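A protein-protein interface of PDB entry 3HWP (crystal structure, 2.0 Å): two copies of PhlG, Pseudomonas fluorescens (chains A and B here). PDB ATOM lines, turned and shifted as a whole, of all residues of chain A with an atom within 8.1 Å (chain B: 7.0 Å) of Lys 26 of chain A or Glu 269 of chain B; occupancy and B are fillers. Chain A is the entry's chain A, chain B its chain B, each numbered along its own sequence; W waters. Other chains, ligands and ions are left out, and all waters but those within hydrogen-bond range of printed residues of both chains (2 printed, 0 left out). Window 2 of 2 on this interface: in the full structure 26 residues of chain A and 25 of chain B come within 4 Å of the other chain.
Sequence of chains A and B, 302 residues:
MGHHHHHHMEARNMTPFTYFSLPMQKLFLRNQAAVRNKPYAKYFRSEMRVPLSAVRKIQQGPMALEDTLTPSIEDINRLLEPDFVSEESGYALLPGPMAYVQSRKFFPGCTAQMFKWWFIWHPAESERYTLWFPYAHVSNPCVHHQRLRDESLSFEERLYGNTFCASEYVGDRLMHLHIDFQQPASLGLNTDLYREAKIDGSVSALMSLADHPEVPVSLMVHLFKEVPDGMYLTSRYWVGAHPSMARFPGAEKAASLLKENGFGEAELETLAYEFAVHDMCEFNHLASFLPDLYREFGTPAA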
ATOM      1  N   PHE A  20      -8.981   5.459 -27.260  1.00  0.00           N
ATOM      2  CA  PHE A  20      -7.942   4.486 -26.898  1.00  0.00           C
ATOM      3  C   PHE A  20      -8.612   3.349 -26.132  1.00  0.00           C
ATOM      4  O   PHE A  20      -9.274   3.594 -25.126  1.00  0.00           O
ATOM      5  CB  PHE A  20      -6.862   5.135 -26.019  1.00  0.00           C
ATOM      6  CG  PHE A  20      -6.179   6.321 -26.660  1.00  0.00           C
ATOM      7  CD1 PHE A  20      -5.253   6.138 -27.666  1.00  0.00           C
ATOM      8  CD2 PHE A  20      -6.475   7.615 -26.253  1.00  0.00           C
ATOM      9  CE1 PHE A  20      -4.628   7.225 -28.267  1.00  0.00           C
ATOM     10  CE2 PHE A  20      -5.854   8.704 -26.834  1.00  0.00           C
ATOM     11  CZ  PHE A  20      -4.932   8.513 -27.849  1.00  0.00           C
ATOM     12  N   SER A  21      -8.458   2.109 -26.590  1.00  0.00           N
ATOM     13  CA  SER A  21      -9.209   1.008 -25.979  1.00  0.00           C
ATOM     14  C   SER A  21      -8.934   0.937 -24.475  1.00  0.00           C
ATOM     15  O   SER A  21      -7.905   1.434 -23.996  1.00  0.00           O
ATOM     16  CB  SER A  21      -8.890  -0.330 -26.657  1.00  0.00           C
ATOM     17  OG  SER A  21      -7.549  -0.741 -26.397  1.00  0.00           O
ATOM     18  N   LEU A  22      -9.853   0.326 -23.729  1.00  0.00           N
ATOM     19  CA  LEU A  22      -9.697   0.229 -22.280  1.00  0.00           C
ATOM     20  C   LEU A  22      -8.327  -0.347 -21.862  1.00  0.00           C
ATOM     21  O   LEU A  22      -7.653   0.226 -21.009  1.00  0.00           O
ATOM     22  CB  LEU A  22     -10.850  -0.566 -21.643  1.00  0.00           C
ATOM     23  CG  LEU A  22     -10.697  -0.848 -20.136  1.00  0.00           C
ATOM     24  CD1 LEU A  22     -10.619   0.429 -19.311  1.00  0.00           C
ATOM     25  CD2 LEU A  22     -11.820  -1.730 -19.630  1.00  0.00           C
ATOM     26  N   PRO A  23      -7.909  -1.477 -22.463  1.00  0.00           N
ATOM     27  CA  PRO A  23      -6.612  -2.063 -22.083  1.00  0.00           C
ATOM     28  C   PRO A  23      -5.454  -1.101 -22.363  1.00  0.00           C
ATOM     29  O   PRO A  23      -4.475  -1.075 -21.627  1.00  0.00           O
ATOM     30  CB  PRO A  23      -6.491  -3.286 -22.995  1.00  0.00           C
ATOM     31  CG  PRO A  23      -7.890  -3.567 -23.475  1.00  0.00           C
ATOM     32  CD  PRO A  23      -8.607  -2.270 -23.491  1.00  0.00           C
ATOM     33  N   MET A  24      -5.571  -0.322 -23.433  1.00  0.00           N
ATOM     34  CA  MET A  24      -4.553   0.662 -23.776  1.00  0.00           C
ATOM     35  C   MET A  24      -4.521   1.852 -22.812  1.00  0.00           C
ATOM     36  O   MET A  24      -3.460   2.396 -22.535  1.00  0.00           O
ATOM     37  CB  MET A  24      -4.730   1.116 -25.228  1.00  0.00           C
ATOM     38  CG  MET A  24      -4.246   0.063 -26.211  1.00  0.00           C
ATOM     39  SD  MET A  24      -4.390   0.538 -28.110  1.00  0.00           S
ATOM     40  CE  MET A  24      -3.678   2.350 -28.076  1.00  0.00           C
ATOM     41  N   GLN A  25      -5.683   2.255 -22.299  1.00  0.00           N
ATOM     42  CA  GLN A  25      -5.720   3.286 -21.264  1.00  0.00           C
ATOM     43  C   GLN A  25      -5.023   2.790 -19.999  1.00  0.00           C
ATOM     44  O   GLN A  25      -4.300   3.539 -19.339  1.00  0.00           O
ATOM     45  CB  GLN A  25      -7.157   3.679 -20.928  1.00  0.00           C
ATOM     46  CG  GLN A  25      -7.888   4.381 -22.063  1.00  0.00           C
ATOM     47  CD  GLN A  25      -9.279   4.821 -21.657  1.00  0.00           C
ATOM     48  OE1 GLN A  25      -9.502   5.261 -20.526  1.00  0.00           O
ATOM     49  NE2 GLN A  25     -10.229   4.710 -22.583  1.00  0.00           N
ATOM     50  N   LYS A  26      -5.243   1.527 -19.661  1.00  0.00           N
ATOM     51  CA  LYS A  26      -4.571   0.950 -18.502  1.00  0.00           C
ATOM     52  C   LYS A  26      -3.063   0.897 -18.731  1.00  0.00           C
ATOM     53  O   LYS A  26      -2.283   1.230 -17.841  1.00  0.00           O
ATOM     54  CB  LYS A  26      -5.133  -0.432 -18.157  1.00  0.00           C
ATOM     55  CG  LYS A  26      -6.596  -0.384 -17.703  1.00  0.00           C
ATOM     56  CD  LYS A  26      -7.127  -1.770 -17.343  1.00  0.00           C
ATOM     57  CE  LYS A  26      -8.535  -1.704 -16.754  1.00  0.00           C
ATOM     58  NZ  LYS A  26      -8.983  -3.046 -16.253  1.00  0.00           N
ATOM     59  N   LEU A  27      -2.653   0.489 -19.927  1.00  0.00           N
ATOM     60  CA  LEU A  27      -1.228   0.467 -20.248  1.00  0.00           C
ATOM     61  C   LEU A  27      -0.611   1.861 -20.116  1.00  0.00           C
ATOM     62  O   LEU A  27       0.535   2.003 -19.670  1.00  0.00           O
ATOM     63  CB  LEU A  27      -0.985  -0.104 -21.651  1.00  0.00           C
ATOM     64  CG  LEU A  27       0.472  -0.079 -22.129  1.00  0.00           C
ATOM     65  CD1 LEU A  27       1.395  -0.804 -21.114  1.00  0.00           C
ATOM     66  CD2 LEU A  27       0.593  -0.707 -23.514  1.00  0.00           C
ATOM     67  N   PHE A  28      -1.371   2.888 -20.488  1.00  0.00           N
ATOM     68  CA  PHE A  28      -0.878   4.263 -20.409  1.00  0.00           C
ATOM     69  C   PHE A  28      -0.482   4.607 -18.977  1.00  0.00           C
ATOM     70  O   PHE A  28       0.594   5.179 -18.735  1.00  0.00           O
ATOM     71  CB  PHE A  28      -1.926   5.267 -20.906  1.00  0.00           C
ATOM     72  CG  PHE A  28      -1.530   6.707 -20.684  1.00  0.00           C
ATOM     73  CD1 PHE A  28      -0.758   7.382 -21.621  1.00  0.00           C
ATOM     74  CD2 PHE A  28      -1.922   7.381 -19.537  1.00  0.00           C
ATOM     75  CE1 PHE A  28      -0.387   8.707 -21.416  1.00  0.00           C
ATOM     76  CE2 PHE A  28      -1.558   8.701 -19.327  1.00  0.00           C
ATOM     77  CZ  PHE A  28      -0.785   9.364 -20.265  1.00  0.00           C
ATOM     78  N   LEU A  29      -1.372   4.280 -18.045  1.00  0.00           N
ATOM     79  CA  LEU A  29      -1.153   4.544 -16.621  1.00  0.00           C
ATOM     80  C   LEU A  29       0.068   3.808 -16.101  1.00  0.00           C
ATOM     81  O   LEU A  29       0.843   4.356 -15.312  1.00  0.00           O
ATOM     82  CB  LEU A  29      -2.388   4.158 -15.804  1.00  0.00           C
ATOM     83  CG  LEU A  29      -3.649   4.946 -16.171  1.00  0.00           C
ATOM     84  CD1 LEU A  29      -4.870   4.367 -15.470  1.00  0.00           C
ATOM     85  CD2 LEU A  29      -3.475   6.421 -15.840  1.00  0.00           C
ATOM     86  N   ARG A  30       0.246   2.567 -16.541  1.00  0.00           N
ATOM     87  CA  ARG A  30       1.434   1.779 -16.192  1.00  0.00           C
ATOM     88  C   ARG A  30       2.704   2.447 -16.721  1.00  0.00           C
ATOM     89  O   ARG A  30       3.690   2.621 -15.995  1.00  0.00           O
ATOM     90  CB  ARG A  30       1.344   0.362 -16.781  1.00  0.00           C
ATOM     91  CG  ARG A  30       0.504  -0.652 -16.007  1.00  0.00           C
ATOM     92  CD  ARG A  30       0.631  -2.025 -16.674  1.00  0.00           C
ATOM     93  NE  ARG A  30       0.405  -3.180 -15.799  1.00  0.00           N
ATOM     94  CZ  ARG A  30       1.367  -4.007 -15.395  1.00  0.00           C
ATOM     95  NH1 ARG A  30       2.616  -3.797 -15.752  1.00  0.00           N
ATOM     96  NH2 ARG A  30       1.090  -5.047 -14.634  1.00  0.00           N
ATOM     97  N   ASN A  31       2.684   2.808 -18.005  1.00  0.00           N
ATOM     98  CA  ASN A  31       3.834   3.443 -18.645  1.00  0.00           C
ATOM     99  C   ASN A  31       4.160   4.806 -18.056  1.00  0.00           C
ATOM    100  O   ASN A  31       5.331   5.181 -17.940  1.00  0.00           O
ATOM    101  CB  ASN A  31       3.615   3.587 -20.155  1.00  0.00           C
ATOM    102  CG  ASN A  31       3.779   2.277 -20.888  1.00  0.00           C
ATOM    103  OD1 ASN A  31       4.385   1.338 -20.372  1.00  0.00           O
ATOM    104  ND2 ASN A  31       3.237   2.203 -22.099  1.00  0.00           N
ATOM    105  N   GLN A  32       3.115   5.538 -17.684  1.00  0.00           N
ATOM    106  CA  GLN A  32       3.260   6.848 -17.066  1.00  0.00           C
ATOM    107  C   GLN A  32       3.986   6.746 -15.728  1.00  0.00           C
ATOM    108  O   GLN A  32       4.835   7.583 -15.404  1.00  0.00           O
ATOM    109  CB  GLN A  32       1.883   7.489 -16.871  1.00  0.00           C
ATOM    110  CG  GLN A  32       1.902   8.863 -16.215  1.00  0.00           C
ATOM    111  CD  GLN A  32       0.508   9.473 -16.127  1.00  0.00           C
ATOM    112  OE1 GLN A  32      -0.435   8.835 -15.647  1.00  0.00           O
ATOM    113  NE2 GLN A  32       0.371  10.706 -16.597  1.00  0.00           N
ATOM    114  N   ALA A  33       3.672   5.713 -14.952  1.00  0.00           N
ATOM    115  CA  ALA A  33       4.389   5.504 -13.690  1.00  0.00           C
ATOM    116  C   ALA A  33       5.849   5.128 -13.943  1.00  0.00           C
ATOM    117  O   ALA A  33       6.772   5.648 -13.298  1.00  0.00           O
ATOM    118  CB  ALA A  33       3.703   4.440 -12.847  1.00  0.00           C
ATOM    119  N   PRO A 134       2.673   5.848 -26.078  1.00  0.00           N
ATOM    120  CA  PRO A 134       2.405   5.694 -24.642  1.00  0.00           C
ATOM    121  C   PRO A 134       1.289   4.694 -24.330  1.00  0.00           C
ATOM    122  O   PRO A 134       1.385   3.998 -23.318  1.00  0.00           O
ATOM    123  CB  PRO A 134       1.982   7.104 -24.221  1.00  0.00           C
ATOM    124  CG  PRO A 134       2.773   7.997 -25.154  1.00  0.00           C
ATOM    125  CD  PRO A 134       2.768   7.267 -26.474  1.00  0.00           C
ATOM    126  N   TYR A 135       0.266   4.617 -25.181  1.00  0.00           N
ATOM    127  CA  TYR A 135      -0.910   3.791 -24.892  1.00  0.00           C
ATOM    128  C   TYR A 135      -0.790   2.344 -25.362  1.00  0.00           C
ATOM    129  O   TYR A 135      -1.622   1.519 -25.001  1.00  0.00           O
ATOM    130  CB  TYR A 135      -2.171   4.383 -25.534  1.00  0.00           C
ATOM    131  CG  TYR A 135      -2.568   5.766 -25.071  1.00  0.00           C
ATOM    132  CD1 TYR A 135      -3.532   5.943 -24.089  1.00  0.00           C
ATOM    133  CD2 TYR A 135      -2.005   6.894 -25.643  1.00  0.00           C
ATOM    134  CE1 TYR A 135      -3.906   7.208 -23.676  1.00  0.00           C
ATOM    135  CE2 TYR A 135      -2.370   8.153 -25.240  1.00  0.00           C
ATOM    136  CZ  TYR A 135      -3.315   8.304 -24.258  1.00  0.00           C
ATOM    137  OH  TYR A 135      -3.672   9.565 -23.860  1.00  0.00           O
ATOM    138  N   TYR A 169       0.112  -3.522 -27.807  1.00  0.00           N
ATOM    139  CA  TYR A 169      -1.285  -3.666 -28.172  1.00  0.00           C
ATOM    140  C   TYR A 169      -1.506  -3.174 -29.591  1.00  0.00           C
ATOM    141  O   TYR A 169      -0.965  -2.135 -29.997  1.00  0.00           O
ATOM    142  CB  TYR A 169      -2.170  -2.852 -27.235  1.00  0.00           C
ATOM    143  CG  TYR A 169      -2.438  -3.517 -25.917  1.00  0.00           C
ATOM    144  CD1 TYR A 169      -3.529  -4.369 -25.755  1.00  0.00           C
ATOM    145  CD2 TYR A 169      -1.605  -3.300 -24.836  1.00  0.00           C
ATOM    146  CE1 TYR A 169      -3.777  -4.977 -24.556  1.00  0.00           C
ATOM    147  CE2 TYR A 169      -1.841  -3.909 -23.625  1.00  0.00           C
ATOM    148  CZ  TYR A 169      -2.928  -4.746 -23.490  1.00  0.00           C
ATOM    149  OH  TYR A 169      -3.170  -5.343 -22.282  1.00  0.00           O
ATOM    150  N   GLN B  59      -9.912   9.253 -21.320  1.00  0.00           N
ATOM    151  CA  GLN B  59      -8.793   8.679 -22.054  1.00  0.00           C
ATOM    152  C   GLN B  59      -7.714   8.082 -21.156  1.00  0.00           C
ATOM    153  O   GLN B  59      -6.774   7.454 -21.643  1.00  0.00           O
ATOM    154  CB  GLN B  59      -8.151   9.734 -22.958  1.00  0.00           C
ATOM    155  CG  GLN B  59      -8.998  10.099 -24.156  1.00  0.00           C
ATOM    156  CD  GLN B  59      -8.408  11.248 -24.934  1.00  0.00           C
ATOM    157  OE1 GLN B  59      -7.452  11.883 -24.490  1.00  0.00           O
ATOM    158  NE2 GLN B  59      -8.982  11.533 -26.093  1.00  0.00           N
ATOM    159  N   GLN B  60      -7.835   8.289 -19.853  1.00  0.00           N
ATOM    160  CA  GLN B  60      -6.792   7.841 -18.937  1.00  0.00           C
ATOM    161  C   GLN B  60      -7.348   6.974 -17.803  1.00  0.00           C
ATOM    162  O   GLN B  60      -7.016   7.163 -16.637  1.00  0.00           O
ATOM    163  CB  GLN B  60      -5.996   9.045 -18.421  1.00  0.00           C
ATOM    164  CG  GLN B  60      -5.489   9.928 -19.578  1.00  0.00           C
ATOM    165  CD  GLN B  60      -4.555  11.049 -19.146  1.00  0.00           C
ATOM    166  OE1 GLN B  60      -4.045  11.062 -18.024  1.00  0.00           O
ATOM    167  NE2 GLN B  60      -4.329  11.998 -20.042  1.00  0.00           N
ATOM    168  N   GLY B  61      -8.196   6.017 -18.165  1.00  0.00           N
ATOM    169  CA  GLY B  61      -8.715   5.056 -17.211  1.00  0.00           C
ATOM    170  C   GLY B  61     -10.041   5.444 -16.580  1.00  0.00           C
ATOM    171  O   GLY B  61     -10.611   6.490 -16.888  1.00  0.00           O
ATOM    172  N   PRO B  62     -10.550   4.583 -15.695  1.00  0.00           N
ATOM    173  CA  PRO B  62     -11.840   4.773 -15.027  1.00  0.00           C
ATOM    174  C   PRO B  62     -11.759   5.792 -13.900  1.00  0.00           C
ATOM    175  O   PRO B  62     -10.660   6.110 -13.427  1.00  0.00           O
ATOM    176  CB  PRO B  62     -12.111   3.387 -14.441  1.00  0.00           C
ATOM    177  CG  PRO B  62     -10.764   2.847 -14.174  1.00  0.00           C
ATOM    178  CD  PRO B  62      -9.995   3.250 -15.409  1.00  0.00           C
ATOM    179  N   TYR B  91     -16.315   7.159 -16.583  1.00  0.00           N
ATOM    180  CA  TYR B  91     -16.834   5.789 -16.541  1.00  0.00           C
ATOM    181  C   TYR B  91     -16.118   4.982 -15.462  1.00  0.00           C
ATOM    182  O   TYR B  91     -15.003   5.326 -15.044  1.00  0.00           O
ATOM    183  CB  TYR B  91     -16.663   5.092 -17.910  1.00  0.00           C
ATOM    184  CG  TYR B  91     -15.215   4.793 -18.245  1.00  0.00           C
ATOM    185  CD1 TYR B  91     -14.641   3.575 -17.893  1.00  0.00           C
ATOM    186  CD2 TYR B  91     -14.409   5.738 -18.879  1.00  0.00           C
ATOM    187  CE1 TYR B  91     -13.306   3.293 -18.167  1.00  0.00           C
ATOM    188  CE2 TYR B  91     -13.063   5.465 -19.168  1.00  0.00           C
ATOM    189  CZ  TYR B  91     -12.521   4.235 -18.800  1.00  0.00           C
ATOM    190  OH  TYR B  91     -11.195   3.929 -19.062  1.00  0.00           O
ATOM    191  N   ALA B  92     -16.753   3.911 -14.999  1.00  0.00           N
ATOM    192  CA  ALA B  92     -16.085   2.990 -14.086  1.00  0.00           C
ATOM    193  C   ALA B  92     -16.806   1.661 -14.012  1.00  0.00           C
ATOM    194  O   ALA B  92     -17.976   1.548 -14.397  1.00  0.00           O
ATOM    195  CB  ALA B  92     -15.951   3.605 -12.677  1.00  0.00           C
ATOM    196  N   LEU B  93     -16.103   0.643 -13.525  1.00  0.00           N
ATOM    197  CA  LEU B  93     -16.769  -0.600 -13.179  1.00  0.00           C
ATOM    198  C   LEU B  93     -17.001  -0.616 -11.666  1.00  0.00           C
ATOM    199  O   LEU B  93     -16.060  -0.457 -10.890  1.00  0.00           O
ATOM    200  CB  LEU B  93     -15.944  -1.804 -13.621  1.00  0.00           C
ATOM    201  CG  LEU B  93     -16.569  -3.134 -13.203  1.00  0.00           C
ATOM    202  CD1 LEU B  93     -17.708  -3.511 -14.142  1.00  0.00           C
ATOM    203  CD2 LEU B  93     -15.496  -4.211 -13.161  1.00  0.00           C
ATOM    204  N   MET B  98     -21.028  -3.882 -12.183  1.00  0.00           N
ATOM    205  CA  MET B  98     -21.898  -2.950 -12.900  1.00  0.00           C
ATOM    206  C   MET B  98     -21.117  -1.853 -13.631  1.00  0.00           C
ATOM    207  O   MET B  98     -20.314  -1.140 -13.029  1.00  0.00           O
ATOM    208  CB  MET B  98     -22.904  -2.357 -11.907  1.00  0.00           C
ATOM    209  CG  MET B  98     -23.839  -1.306 -12.449  1.00  0.00           C
ATOM    210  SD  MET B  98     -25.385  -1.139 -11.258  1.00  0.00           S
ATOM    211  CE  MET B  98     -26.501  -2.394 -12.153  1.00  0.00           C
ATOM    212  N   ALA B  99     -21.336  -1.741 -14.942  1.00  0.00           N
ATOM    213  CA  ALA B  99     -20.786  -0.626 -15.714  1.00  0.00           C
ATOM    214  C   ALA B  99     -21.493   0.671 -15.311  1.00  0.00           C
ATOM    215  O   ALA B  99     -22.704   0.682 -15.085  1.00  0.00           O
ATOM    216  CB  ALA B  99     -20.949  -0.875 -17.222  1.00  0.00           C
ATOM    217  N   GLY B 264     -18.653 -10.735 -17.972  1.00  0.00           N
ATOM    218  CA  GLY B 264     -17.871 -10.711 -16.754  1.00  0.00           C
ATOM    219  C   GLY B 264     -17.388  -9.306 -16.441  1.00  0.00           C
ATOM    220  O   GLY B 264     -17.725  -8.350 -17.146  1.00  0.00           O
ATOM    221  N   GLU B 265     -16.596  -9.184 -15.379  1.00  0.00           N
ATOM    222  CA  GLU B 265     -16.016  -7.906 -14.983  1.00  0.00           C
ATOM    223  C   GLU B 265     -15.315  -7.190 -16.136  1.00  0.00           C
ATOM    224  O   GLU B 265     -15.504  -5.987 -16.336  1.00  0.00           O
ATOM    225  CB  GLU B 265     -15.005  -8.116 -13.852  1.00  0.00           C
ATOM    226  CG  GLU B 265     -15.632  -8.345 -12.495  1.00  0.00           C
ATOM    227  CD  GLU B 265     -15.896  -9.809 -12.227  1.00  0.00           C
ATOM    228  OE1 GLU B 265     -15.897 -10.610 -13.187  1.00  0.00           O
ATOM    229  OE2 GLU B 265     -16.084 -10.159 -11.049  1.00  0.00           O
ATOM    230  N   ALA B 266     -14.486  -7.923 -16.876  1.00  0.00           N
ATOM    231  CA  ALA B 266     -13.694  -7.317 -17.943  1.00  0.00           C
ATOM    232  C   ALA B 266     -14.593  -6.767 -19.043  1.00  0.00           C
ATOM    233  O   ALA B 266     -14.384  -5.654 -19.542  1.00  0.00           O
ATOM    234  CB  ALA B 266     -12.710  -8.328 -18.520  1.00  0.00           C
ATOM    235  N   GLU B 267     -15.596  -7.556 -19.414  1.00  0.00           N
ATOM    236  CA  GLU B 267     -16.514  -7.160 -20.470  1.00  0.00           C
ATOM    237  C   GLU B 267     -17.337  -5.945 -20.045  1.00  0.00           C
ATOM    238  O   GLU B 267     -17.601  -5.048 -20.849  1.00  0.00           O
ATOM    239  CB  GLU B 267     -17.414  -8.329 -20.868  1.00  0.00           C
ATOM    240  CG  GLU B 267     -16.673  -9.476 -21.545  1.00  0.00           C
ATOM    241  CD  GLU B 267     -15.893 -10.341 -20.561  1.00  0.00           C
ATOM    242  OE1 GLU B 267     -16.267 -10.378 -19.366  1.00  0.00           O
ATOM    243  OE2 GLU B 267     -14.897 -10.980 -20.984  1.00  0.00           O
ATOM    244  N   LEU B 268     -17.719  -5.899 -18.775  1.00  0.00           N
ATOM    245  CA  LEU B 268     -18.518  -4.780 -18.285  1.00  0.00           C
ATOM    246  C   LEU B 268     -17.700  -3.490 -18.124  1.00  0.00           C
ATOM    247  O   LEU B 268     -18.216  -2.395 -18.355  1.00  0.00           O
ATOM    248  CB  LEU B 268     -19.251  -5.152 -16.989  1.00  0.00           C
ATOM    249  CG  LEU B 268     -20.390  -6.171 -17.174  1.00  0.00           C
ATOM    250  CD1 LEU B 268     -20.882  -6.735 -15.844  1.00  0.00           C
ATOM    251  CD2 LEU B 268     -21.559  -5.569 -17.956  1.00  0.00           C
ATOM    252  N   GLU B 269     -16.431  -3.607 -17.736  1.00  0.00           N
ATOM    253  CA  GLU B 269     -15.599  -2.408 -17.609  1.00  0.00           C
ATOM    254  C   GLU B 269     -15.354  -1.820 -18.996  1.00  0.00           C
ATOM    255  O   GLU B 269     -15.406  -0.606 -19.196  1.00  0.00           O
ATOM    256  CB  GLU B 269     -14.269  -2.685 -16.884  1.00  0.00           C
ATOM    257  CG  GLU B 269     -13.511  -1.395 -16.595  1.00  0.00           C
ATOM    258  CD  GLU B 269     -12.253  -1.554 -15.744  1.00  0.00           C
ATOM    259  OE1 GLU B 269     -11.704  -2.676 -15.628  1.00  0.00           O
ATOM    260  OE2 GLU B 269     -11.796  -0.518 -15.209  1.00  0.00           O
ATOM    261  N   THR B 270     -15.091  -2.696 -19.955  1.00  0.00           N
ATOM    262  CA  THR B 270     -14.991  -2.299 -21.349  1.00  0.00           C
ATOM    263  C   THR B 270     -16.288  -1.641 -21.820  1.00  0.00           C
ATOM    264  O   THR B 270     -16.270  -0.585 -22.441  1.00  0.00           O
ATOM    265  CB  THR B 270     -14.725  -3.519 -22.242  1.00  0.00           C
ATOM    266  OG1 THR B 270     -13.392  -3.993 -22.011  1.00  0.00           O
ATOM    267  CG2 THR B 270     -14.890  -3.147 -23.718  1.00  0.00           C
ATOM    268  N   LEU B 271     -17.410  -2.286 -21.531  1.00  0.00           N
ATOM    269  CA  LEU B 271     -18.716  -1.757 -21.905  1.00  0.00           C
ATOM    270  C   LEU B 271     -18.949  -0.382 -21.285  1.00  0.00           C
ATOM    271  O   LEU B 271     -19.580   0.467 -21.894  1.00  0.00           O
ATOM    272  CB  LEU B 271     -19.819  -2.732 -21.487  1.00  0.00           C
ATOM    273  CG  LEU B 271     -21.237  -2.555 -22.028  1.00  0.00           C
ATOM    274  CD1 LEU B 271     -21.294  -2.825 -23.534  1.00  0.00           C
ATOM    275  CD2 LEU B 271     -22.187  -3.478 -21.276  1.00  0.00           C
ATOM    276  N   ALA B 272     -18.442  -0.160 -20.073  1.00  0.00           N
ATOM    277  CA  ALA B 272     -18.607   1.140 -19.432  1.00  0.00           C
ATOM    278  C   ALA B 272     -17.909   2.247 -20.235  1.00  0.00           C
ATOM    279  O   ALA B 272     -18.460   3.338 -20.404  1.00  0.00           O
ATOM    280  CB  ALA B 272     -18.105   1.111 -17.994  1.00  0.00           C
ATOM    281  N   TYR B 273     -16.699   1.968 -20.726  1.00  0.00           N
ATOM    282  CA  TYR B 273     -16.005   2.923 -21.589  1.00  0.00           C
ATOM    283  C   TYR B 273     -16.701   3.079 -22.944  1.00  0.00           C
ATOM    284  O   TYR B 273     -16.856   4.200 -23.434  1.00  0.00           O
ATOM    285  CB  TYR B 273     -14.516   2.562 -21.782  1.00  0.00           C
ATOM    286  CG  TYR B 273     -13.811   3.410 -22.835  1.00  0.00           C
ATOM    287  CD1 TYR B 273     -13.683   4.784 -22.680  1.00  0.00           C
ATOM    288  CD2 TYR B 273     -13.274   2.831 -23.984  1.00  0.00           C
ATOM    289  CE1 TYR B 273     -13.044   5.562 -23.642  1.00  0.00           C
ATOM    290  CE2 TYR B 273     -12.631   3.600 -24.946  1.00  0.00           C
ATOM    291  CZ  TYR B 273     -12.521   4.965 -24.767  1.00  0.00           C
ATOM    292  OH  TYR B 273     -11.901   5.734 -25.728  1.00  0.00           O
ATOM    293  N   GLU B 274     -17.119   1.973 -23.556  1.00  0.00           N
ATOM    294  CA  GLU B 274     -17.734   2.068 -24.875  1.00  0.00           C
ATOM    295  C   GLU B 274     -19.085   2.802 -24.809  1.00  0.00           C
ATOM    296  O   GLU B 274     -19.445   3.530 -25.737  1.00  0.00           O
ATOM    297  CB  GLU B 274     -17.865   0.692 -25.535  1.00  0.00           C
ATOM    298  CG  GLU B 274     -16.543  -0.077 -25.685  1.00  0.00           C
ATOM    299  CD  GLU B 274     -15.600   0.519 -26.727  1.00  0.00           C
ATOM    300  OE1 GLU B 274     -16.027   1.394 -27.511  1.00  0.00           O
ATOM    301  OE2 GLU B 274     -14.417   0.106 -26.764  1.00  0.00           O
HETATM  302  O   HOH W   1     -12.263  -0.652 -24.906  1.00  0.00           O
HETATM  303  O   HOH W   2      -1.792  12.339 -17.101  1.00  0.00           O
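N of Phe 20 of chain A lies within hydrogen-bond range of OH of Tyr 273 of chain B.
The side-chain amide oxygen (OE1) of Gln 25 of chain A is in hydrogen-bond range of the side-chain hydroxyl (OH) of Tyr 91 of chain B (2.6 Å).
The side-chain amide oxygen (OE1) of Gln 25 of chain A lies within hydrogen-bond range of the backbone NH (N) of Gly 61 of chain B, at 2.8 Å.
The side-chain amino group (NZ) of Lys 26 of chain A lies within salt-bridge range of the side-chain carboxylate (OE1) of Glu 269 of chain B (2.8 Å).
Water W2 lies within hydrogen-bond range of the side-chain amide oxygen of Gln 60 of chain B (2.7 Å) and the side-chain amide nitrogen of Gln 32 of chain A (2.8 Å).
Water W1 bridges N of Leu 22 of chain A (2.9 Å) and OE2 of Glu 274 of chain B (2.9 Å).
Among the printed residues, pairs that only touch across the chains: Leu 22 of chain A with Tyr 91 of chain B, Leu 22 of chain A with Glu 269 of chain B, Leu 22 of chain A with Thr 270 of chain B, Gln 25 of chain A with Gln 59 of chain B, Gln 25 of chain A with Gln 60 of chain B, Gln 25 of chain A with Tyr 273 of chain B, Phe 28 of chain A with Gln 60 of chain B, Leu 29 of chain A with Gln 60 of chain B and Tyr 135 of chain A with Gln 59 of chain B.
The backbone carbonyl oxygen of Gly 61 of chain B lies close to the side-chain hydroxyl of Tyr 91 of chain B, at 3.4 Å.
The backbone carbonyl oxygen of Ala 266 of chain B sits at hydrogen-bond distance from the side-chain hydroxyl of Thr 270 of chain B (3.1 Å).
NE2 of Gln 25 of chain A sits at hydrogen-bond distance from O of Phe 20 of chain A (2.9 Å).
No position is printed for both chains.
Of the 13 pairs that touch across the chains among the printed residues, none has its exchanged pair printed and touching as well.
Along chain B the printed residues that touch a printed residue of chain A span positions 59 to 273.
Of the 17 printed residues of chain A, 7 touch a printed residue of chain B.
Along chain A the printed residues that touch a printed residue of chain B span positions 20 to 135.
Among the printed residues, 13 pairs touch across the chains.
Among the printed residues, Asp or Glu carboxylates within 4 Å of a Lys or Arg side-chain nitrogen of the other chain: Lys 26 of chain A with Glu 269 of chain B.
Of the printed residues of chain B, Leu 22 of chain A touches Tyr 91 (3.6 Å), Glu 269 (3.5 Å) and Thr 270 (3.4 Å).
Lys 26 of chain A touches just one residue of chain B: Glu 269 (2.8 Å).
Of the printed residues of chain A, Gly 61 of chain B touches Gln 25 (2.8 Å).
Pro 62 of chain B touches none of the printed residues of chain A.
Printed residues of chain A within 4 Å of Tyr 91 of chain B: Leu 22 (3.6 Å) and Gln 25 (2.6 Å).
Ala 99 of chain B touches none of the printed residues of chain A.
Glu 269 of chain B touches just these residues of chain A: Leu 22 (3.5 Å) and Lys 26 (2.8 Å).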
